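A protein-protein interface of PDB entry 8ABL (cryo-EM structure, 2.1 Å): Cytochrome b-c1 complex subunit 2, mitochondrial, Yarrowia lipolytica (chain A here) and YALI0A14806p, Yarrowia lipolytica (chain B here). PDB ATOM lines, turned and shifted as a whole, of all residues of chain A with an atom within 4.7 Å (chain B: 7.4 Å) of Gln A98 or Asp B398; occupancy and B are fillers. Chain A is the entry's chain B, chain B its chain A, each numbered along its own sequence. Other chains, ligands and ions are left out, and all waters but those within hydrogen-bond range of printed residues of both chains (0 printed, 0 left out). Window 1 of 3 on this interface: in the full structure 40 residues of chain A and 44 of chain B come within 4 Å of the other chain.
OH of Tyr A85 lies within hydrogen-bond range of OE1 of Gln A98, at 3.2 Å. The backbone carbonyl oxygen of Lys A83 lies within hydrogen-bond range of the backbone NH of Gln A98 (2.9 Å). OD1 of Asp A36 is in hydrogen-bond range of NE2 of Gln A98 (3.2 Å).
Among the printed residues, merely in contact across the chains: Ile A34 with Leu B394 (3.6 Å), Ile A34 with Leu B395 (3.0 Å), Gly A81 with Ala B391 (3.6 Å), Gly A81 with Leu B395 (3.3 Å), Lys A83 with Leu B395 (3.5 Å), Gln A98 with Leu B395 (3.7 Å) and Gln A98 with Asp B398 (3.9 Å).
Gln A98 touches two residues of chain B. Printed residues of chain A within 4 Å of Asp B398: Gln A98 (3.9 Å). Printed residues of chain B within 4 Å of Ile A34: Leu B394 (3.6 Å) and Leu B395 (3.0 Å). Printed residues of chain A within 4 Å of Ala B391: Gly A81. Of the printed residues of chain B, Gly A81 touches Ala B391 (3.6 Å) and Leu B395 (3.3 Å). Of the printed residues of chain A, Leu B395 touches Ile A34 (3.0 Å), Gly A81 (3.3 Å), Lys A83 (3.5 Å) and Gln A98 (3.7 Å). Tyr A85 touches none of the printed residues of chain B. The nearest residue of chain B that does not touch Gln A98 is Ser B396 (5.8 Å). The nearest printed residue of chain A that does not touch Asp B398 is Ile A34 (5.6 Å).
Of the 12 printed residues of chain B, 4 touch a printed residue of chain A. Hydrophobic or aromatic side chains of chain B within 4 Å of the printed part of chain A: Ala B391, Leu B394 and Leu B395. Of the 11 printed residues of chain A, 4 touch a printed residue of chain B. Hydrophobic or aromatic side chains of chain A within 4 Å of the printed part of chain B: Ile A34. Among the printed residues, 7 pairs touch across the chains. Among the printed residues, no Asp or Glu carboxylate lies within 4 Å of a Lys or Arg side-chain nitrogen of the other chain.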
ATOM      1  N   ILE A  34      22.201 -23.190 -17.716  1.00  0.00           N
ATOM      2  CA  ILE A  34      23.335 -23.211 -16.800  1.00  0.00           C
ATOM      3  C   ILE A  34      23.121 -22.251 -15.637  1.00  0.00           C
ATOM      4  O   ILE A  34      22.993 -21.053 -15.855  1.00  0.00           O
ATOM      5  CB  ILE A  34      24.593 -22.804 -17.583  1.00  0.00           C
ATOM      6  CG1 ILE A  34      24.870 -23.775 -18.732  1.00  0.00           C
ATOM      7  CG2 ILE A  34      25.798 -22.606 -16.675  1.00  0.00           C
ATOM      8  CD1 ILE A  34      24.822 -25.233 -18.322  1.00  0.00           C
ATOM      9  N   SER A  35      23.196 -22.759 -14.407  1.00  0.00           N
ATOM     10  CA  SER A  35      23.117 -21.920 -13.223  1.00  0.00           C
ATOM     11  C   SER A  35      24.482 -21.811 -12.557  1.00  0.00           C
ATOM     12  O   SER A  35      25.242 -22.778 -12.519  1.00  0.00           O
ATOM     13  CB  SER A  35      22.130 -22.491 -12.271  1.00  0.00           C
ATOM     14  OG  SER A  35      20.844 -22.463 -12.844  1.00  0.00           O
ATOM     15  N   ASP A  36      24.756 -20.641 -11.982  1.00  0.00           N
ATOM     16  CA  ASP A  36      25.921 -20.487 -11.130  1.00  0.00           C
ATOM     17  C   ASP A  36      25.454 -20.188  -9.710  1.00  0.00           C
ATOM     18  O   ASP A  36      24.697 -19.253  -9.491  1.00  0.00           O
ATOM     19  CB  ASP A  36      26.808 -19.332 -11.580  1.00  0.00           C
ATOM     20  CG  ASP A  36      27.343 -19.389 -13.000  1.00  0.00           C
ATOM     21  OD1 ASP A  36      27.104 -20.389 -13.698  1.00  0.00           O
ATOM     22  OD2 ASP A  36      27.978 -18.404 -13.402  1.00  0.00           O
ATOM     23  N   GLY A  81      28.126 -33.170 -14.278  1.00  0.00           N
ATOM     24  CA  GLY A  81      28.914 -32.331 -15.166  1.00  0.00           C
ATOM     25  C   GLY A  81      29.143 -30.935 -14.592  1.00  0.00           C
ATOM     26  O   GLY A  81      29.423 -30.009 -15.343  1.00  0.00           O
ATOM     27  N   GLY A  82      29.021 -30.779 -13.269  1.00  0.00           N
ATOM     28  CA  GLY A  82      29.224 -29.477 -12.654  1.00  0.00           C
ATOM     29  C   GLY A  82      30.701 -29.100 -12.598  1.00  0.00           C
ATOM     30  O   GLY A  82      31.569 -29.951 -12.761  1.00  0.00           O
ATOM     31  N   LYS A  83      30.975 -27.824 -12.320  1.00  0.00           N
ATOM     32  CA  LYS A  83      32.336 -27.373 -12.099  1.00  0.00           C
ATOM     33  C   LYS A  83      32.385 -26.546 -10.825  1.00  0.00           C
ATOM     34  O   LYS A  83      31.375 -25.987 -10.399  1.00  0.00           O
ATOM     35  CB  LYS A  83      32.808 -26.431 -13.204  1.00  0.00           C
ATOM     36  CG  LYS A  83      32.616 -26.863 -14.647  1.00  0.00           C
ATOM     37  CD  LYS A  83      33.661 -27.829 -15.178  1.00  0.00           C
ATOM     38  CE  LYS A  83      34.268 -27.420 -16.511  1.00  0.00           C
ATOM     39  NZ  LYS A  83      33.373 -26.553 -17.319  1.00  0.00           N
ATOM     40  N   TYR A  85      34.704 -23.517  -8.741  1.00  0.00           N
ATOM     41  CA  TYR A  85      35.678 -22.446  -8.837  1.00  0.00           C
ATOM     42  C   TYR A  85      35.763 -21.804  -7.468  1.00  0.00           C
ATOM     43  O   TYR A  85      34.741 -21.585  -6.826  1.00  0.00           O
ATOM     44  CB  TYR A  85      35.185 -21.372  -9.806  1.00  0.00           C
ATOM     45  CG  TYR A  85      34.825 -21.883 -11.173  1.00  0.00           C
ATOM     46  CD1 TYR A  85      33.546 -22.349 -11.450  1.00  0.00           C
ATOM     47  CD2 TYR A  85      35.764 -21.901 -12.194  1.00  0.00           C
ATOM     48  CE1 TYR A  85      33.218 -22.834 -12.708  1.00  0.00           C
ATOM     49  CE2 TYR A  85      35.446 -22.376 -13.459  1.00  0.00           C
ATOM     50  CZ  TYR A  85      34.166 -22.840 -13.720  1.00  0.00           C
ATOM     51  OH  TYR A  85      33.847 -23.329 -14.957  1.00  0.00           O
ATOM     52  N   ARG A  96      32.278 -20.994  -5.947  1.00  0.00           N
ATOM     53  CA  ARG A  96      31.259 -20.943  -6.971  1.00  0.00           C
ATOM     54  C   ARG A  96      31.106 -22.324  -7.590  1.00  0.00           C
ATOM     55  O   ARG A  96      32.092 -23.000  -7.876  1.00  0.00           O
ATOM     56  CB  ARG A  96      31.695 -19.963  -8.057  1.00  0.00           C
ATOM     57  CG  ARG A  96      30.684 -19.887  -9.190  1.00  0.00           C
ATOM     58  CD  ARG A  96      30.813 -18.746 -10.172  1.00  0.00           C
ATOM     59  NE  ARG A  96      31.534 -19.126 -11.373  1.00  0.00           N
ATOM     60  CZ  ARG A  96      32.804 -18.832 -11.584  1.00  0.00           C
ATOM     61  NH1 ARG A  96      33.486 -18.165 -10.666  1.00  0.00           N
ATOM     62  NH2 ARG A  96      33.380 -19.199 -12.711  1.00  0.00           N
ATOM     63  N   THR A  97      29.864 -22.689  -7.892  1.00  0.00           N
ATOM     64  CA  THR A  97      29.632 -23.899  -8.652  1.00  0.00           C
ATOM     65  C   THR A  97      28.808 -23.582  -9.887  1.00  0.00           C
ATOM     66  O   THR A  97      27.848 -22.825  -9.820  1.00  0.00           O
ATOM     67  CB  THR A  97      28.848 -24.917  -7.823  1.00  0.00           C
ATOM     68  OG1 THR A  97      27.729 -24.219  -7.282  1.00  0.00           O
ATOM     69  CG2 THR A  97      29.674 -25.510  -6.708  1.00  0.00           C
ATOM     70  N   GLN A  98      29.076 -24.296 -10.975  1.00  0.00           N
ATOM     71  CA  GLN A  98      28.331 -24.098 -12.199  1.00  0.00           C
ATOM     72  C   GLN A  98      27.710 -25.434 -12.570  1.00  0.00           C
ATOM     73  O   GLN A  98      28.406 -26.439 -12.544  1.00  0.00           O
ATOM     74  CB  GLN A  98      29.362 -23.658 -13.225  1.00  0.00           C
ATOM     75  CG  GLN A  98      28.748 -23.143 -14.504  1.00  0.00           C
ATOM     76  CD  GLN A  98      29.795 -22.465 -15.348  1.00  0.00           C
ATOM     77  OE1 GLN A  98      30.804 -23.058 -15.726  1.00  0.00           O
ATOM     78  NE2 GLN A  98      29.559 -21.197 -15.643  1.00  0.00           N
ATOM     79  N   PHE A  99      26.413 -25.458 -12.869  1.00  0.00           N
ATOM     80  CA  PHE A  99      25.739 -26.734 -13.063  1.00  0.00           C
ATOM     81  C   PHE A  99      24.515 -26.512 -13.942  1.00  0.00           C
ATOM     82  O   PHE A  99      24.242 -25.384 -14.325  1.00  0.00           O
ATOM     83  CB  PHE A  99      25.361 -27.351 -11.710  1.00  0.00           C
ATOM     84  CG  PHE A  99      24.708 -26.379 -10.765  1.00  0.00           C
ATOM     85  CD1 PHE A  99      25.492 -25.578  -9.947  1.00  0.00           C
ATOM     86  CD2 PHE A  99      23.327 -26.225 -10.725  1.00  0.00           C
ATOM     87  CE1 PHE A  99      24.913 -24.631  -9.120  1.00  0.00           C
ATOM     88  CE2 PHE A  99      22.744 -25.288  -9.885  1.00  0.00           C
ATOM     89  CZ  PHE A  99      23.542 -24.483  -9.100  1.00  0.00           C
ATOM     90  N   VAL B  49      21.975  -9.127 -20.202  1.00  0.00           N
ATOM     91  CA  VAL B  49      23.288  -8.496 -20.274  1.00  0.00           C
ATOM     92  C   VAL B  49      23.179  -7.133 -20.952  1.00  0.00           C
ATOM     93  O   VAL B  49      22.167  -6.820 -21.576  1.00  0.00           O
ATOM     94  CB  VAL B  49      24.351  -9.381 -20.951  1.00  0.00           C
ATOM     95  CG1 VAL B  49      24.660 -10.634 -20.147  1.00  0.00           C
ATOM     96  CG2 VAL B  49      23.991  -9.670 -22.396  1.00  0.00           C
ATOM     97  N   ALA B 391      26.325 -31.685 -19.871  1.00  0.00           N
ATOM     98  CA  ALA B 391      26.497 -30.413 -19.192  1.00  0.00           C
ATOM     99  C   ALA B 391      27.620 -29.599 -19.828  1.00  0.00           C
ATOM    100  O   ALA B 391      27.435 -28.415 -20.088  1.00  0.00           O
ATOM    101  CB  ALA B 391      26.727 -30.639 -17.720  1.00  0.00           C
ATOM    102  N   LEU B 394      27.063 -27.281 -22.795  1.00  0.00           N
ATOM    103  CA  LEU B 394      26.262 -26.109 -22.492  1.00  0.00           C
ATOM    104  C   LEU B 394      27.043 -25.144 -21.603  1.00  0.00           C
ATOM    105  O   LEU B 394      26.875 -23.934 -21.747  1.00  0.00           O
ATOM    106  CB  LEU B 394      24.964 -26.562 -21.819  1.00  0.00           C
ATOM    107  CG  LEU B 394      24.162 -27.611 -22.587  1.00  0.00           C
ATOM    108  CD1 LEU B 394      22.974 -28.085 -21.769  1.00  0.00           C
ATOM    109  CD2 LEU B 394      23.704 -27.093 -23.944  1.00  0.00           C
ATOM    110  N   LEU B 395      27.856 -25.696 -20.680  1.00  0.00           N
ATOM    111  CA  LEU B 395      28.536 -24.934 -19.629  1.00  0.00           C
ATOM    112  C   LEU B 395      29.512 -23.942 -20.254  1.00  0.00           C
ATOM    113  O   LEU B 395      29.587 -22.784 -19.836  1.00  0.00           O
ATOM    114  CB  LEU B 395      29.311 -25.852 -18.669  1.00  0.00           C
ATOM    115  CG  LEU B 395      28.595 -26.514 -17.490  1.00  0.00           C
ATOM    116  CD1 LEU B 395      29.578 -26.863 -16.388  1.00  0.00           C
ATOM    117  CD2 LEU B 395      27.478 -25.664 -16.938  1.00  0.00           C
ATOM    118  N   SER B 396      30.223 -24.425 -21.285  1.00  0.00           N
ATOM    119  CA  SER B 396      31.207 -23.676 -22.045  1.00  0.00           C
ATOM    120  C   SER B 396      30.698 -22.289 -22.456  1.00  0.00           C
ATOM    121  O   SER B 396      31.456 -21.317 -22.428  1.00  0.00           O
ATOM    122  CB  SER B 396      31.685 -24.486 -23.223  1.00  0.00           C
ATOM    123  OG  SER B 396      30.621 -25.219 -23.820  1.00  0.00           O
ATOM    124  N   LEU B 397      29.397 -22.180 -22.759  1.00  0.00           N
ATOM    125  CA  LEU B 397      28.834 -20.938 -23.268  1.00  0.00           C
ATOM    126  C   LEU B 397      28.372 -20.076 -22.095  1.00  0.00           C
ATOM    127  O   LEU B 397      27.177 -20.063 -21.790  1.00  0.00           O
ATOM    128  CB  LEU B 397      27.661 -21.247 -24.208  1.00  0.00           C
ATOM    129  CG  LEU B 397      27.641 -22.645 -24.822  1.00  0.00           C
ATOM    130  CD1 LEU B 397      26.251 -23.090 -25.246  1.00  0.00           C
ATOM    131  CD2 LEU B 397      28.635 -22.765 -25.967  1.00  0.00           C
ATOM    132  N   ASP B 398      29.300 -19.338 -21.462  1.00  0.00           N
ATOM    133  CA  ASP B 398      28.950 -18.598 -20.250  1.00  0.00           C
ATOM    134  C   ASP B 398      29.128 -17.079 -20.356  1.00  0.00           C
ATOM    135  O   ASP B 398      29.004 -16.392 -19.343  1.00  0.00           O
ATOM    136  CB  ASP B 398      29.611 -19.200 -19.001  1.00  0.00           C
ATOM    137  CG  ASP B 398      31.098 -19.439 -19.170  1.00  0.00           C
ATOM    138  OD1 ASP B 398      31.858 -18.461 -19.059  1.00  0.00           O
ATOM    139  OD2 ASP B 398      31.483 -20.591 -19.401  1.00  0.00           O
ATOM    140  N   GLY B 399      29.406 -16.548 -21.557  1.00  0.00           N
ATOM    141  CA  GLY B 399      29.429 -15.109 -21.814  1.00  0.00           C
ATOM    142  C   GLY B 399      29.134 -14.803 -23.282  1.00  0.00           C
ATOM    143  O   GLY B 399      29.111 -15.734 -24.075  1.00  0.00           O
ATOM    144  N   THR B 400      28.954 -13.524 -23.642  1.00  0.00           N
ATOM    145  CA  THR B 400      28.506 -13.176 -24.985  1.00  0.00           C
ATOM    146  C   THR B 400      29.539 -13.552 -26.045  1.00  0.00           C
ATOM    147  O   THR B 400      29.165 -13.947 -27.146  1.00  0.00           O
ATOM    148  CB  THR B 400      28.111 -11.703 -25.133  1.00  0.00           C
ATOM    149  OG1 THR B 400      29.306 -10.931 -25.134  1.00  0.00           O
ATOM    150  CG2 THR B 400      27.172 -11.245 -24.047  1.00  0.00           C
ATOM    151  N   THR B 401      30.825 -13.471 -25.695  1.00  0.00           N
ATOM    152  CA  THR B 401      31.869 -13.822 -26.639  1.00  0.00           C
ATOM    153  C   THR B 401      31.848 -15.330 -26.873  1.00  0.00           C
ATOM    154  O   THR B 401      32.047 -15.782 -27.995  1.00  0.00           O
ATOM    155  CB  THR B 401      33.234 -13.248 -26.243  1.00  0.00           C
ATOM    156  OG1 THR B 401      33.077 -11.829 -26.164  1.00  0.00           O
ATOM    157  CG2 THR B 401      34.305 -13.568 -27.263  1.00  0.00           C
ATOM    158  N   TYR B 402      31.614 -16.103 -25.803  1.00  0.00           N
ATOM    159  CA  TYR B 402      31.559 -17.553 -25.924  1.00  0.00           C
ATOM    160  C   TYR B 402      30.375 -17.967 -26.784  1.00  0.00           C
ATOM    161  O   TYR B 402      30.493 -18.871 -27.607  1.00  0.00           O
ATOM    162  CB  TYR B 402      31.534 -18.248 -24.567  1.00  0.00           C
ATOM    163  CG  TYR B 402      32.822 -18.100 -23.808  1.00  0.00           C
ATOM    164  CD1 TYR B 402      34.024 -18.577 -24.316  1.00  0.00           C
ATOM    165  CD2 TYR B 402      32.836 -17.448 -22.589  1.00  0.00           C
ATOM    166  CE1 TYR B 402      35.210 -18.421 -23.615  1.00  0.00           C
ATOM    167  CE2 TYR B 402      34.016 -17.280 -21.878  1.00  0.00           C
ATOM    168  CZ  TYR B 402      35.205 -17.773 -22.391  1.00  0.00           C
ATOM    169  OH  TYR B 402      36.369 -17.616 -21.694  1.00  0.00           O
ATOM    170  N   VAL B 403      29.253 -17.277 -26.604  1.00  0.00           N
ATOM    171  CA  VAL B 403      28.058 -17.595 -27.363  1.00  0.00           C
ATOM    172  C   VAL B 403      28.300 -17.237 -28.826  1.00  0.00           C
ATOM    173  O   VAL B 403      27.991 -18.040 -29.697  1.00  0.00           O
ATOM    174  CB  VAL B 403      26.800 -16.931 -26.774  1.00  0.00           C
ATOM    175  CG1 VAL B 403      25.581 -17.083 -27.665  1.00  0.00           C
ATOM    176  CG2 VAL B 403      26.488 -17.480 -25.394  1.00  0.00           C
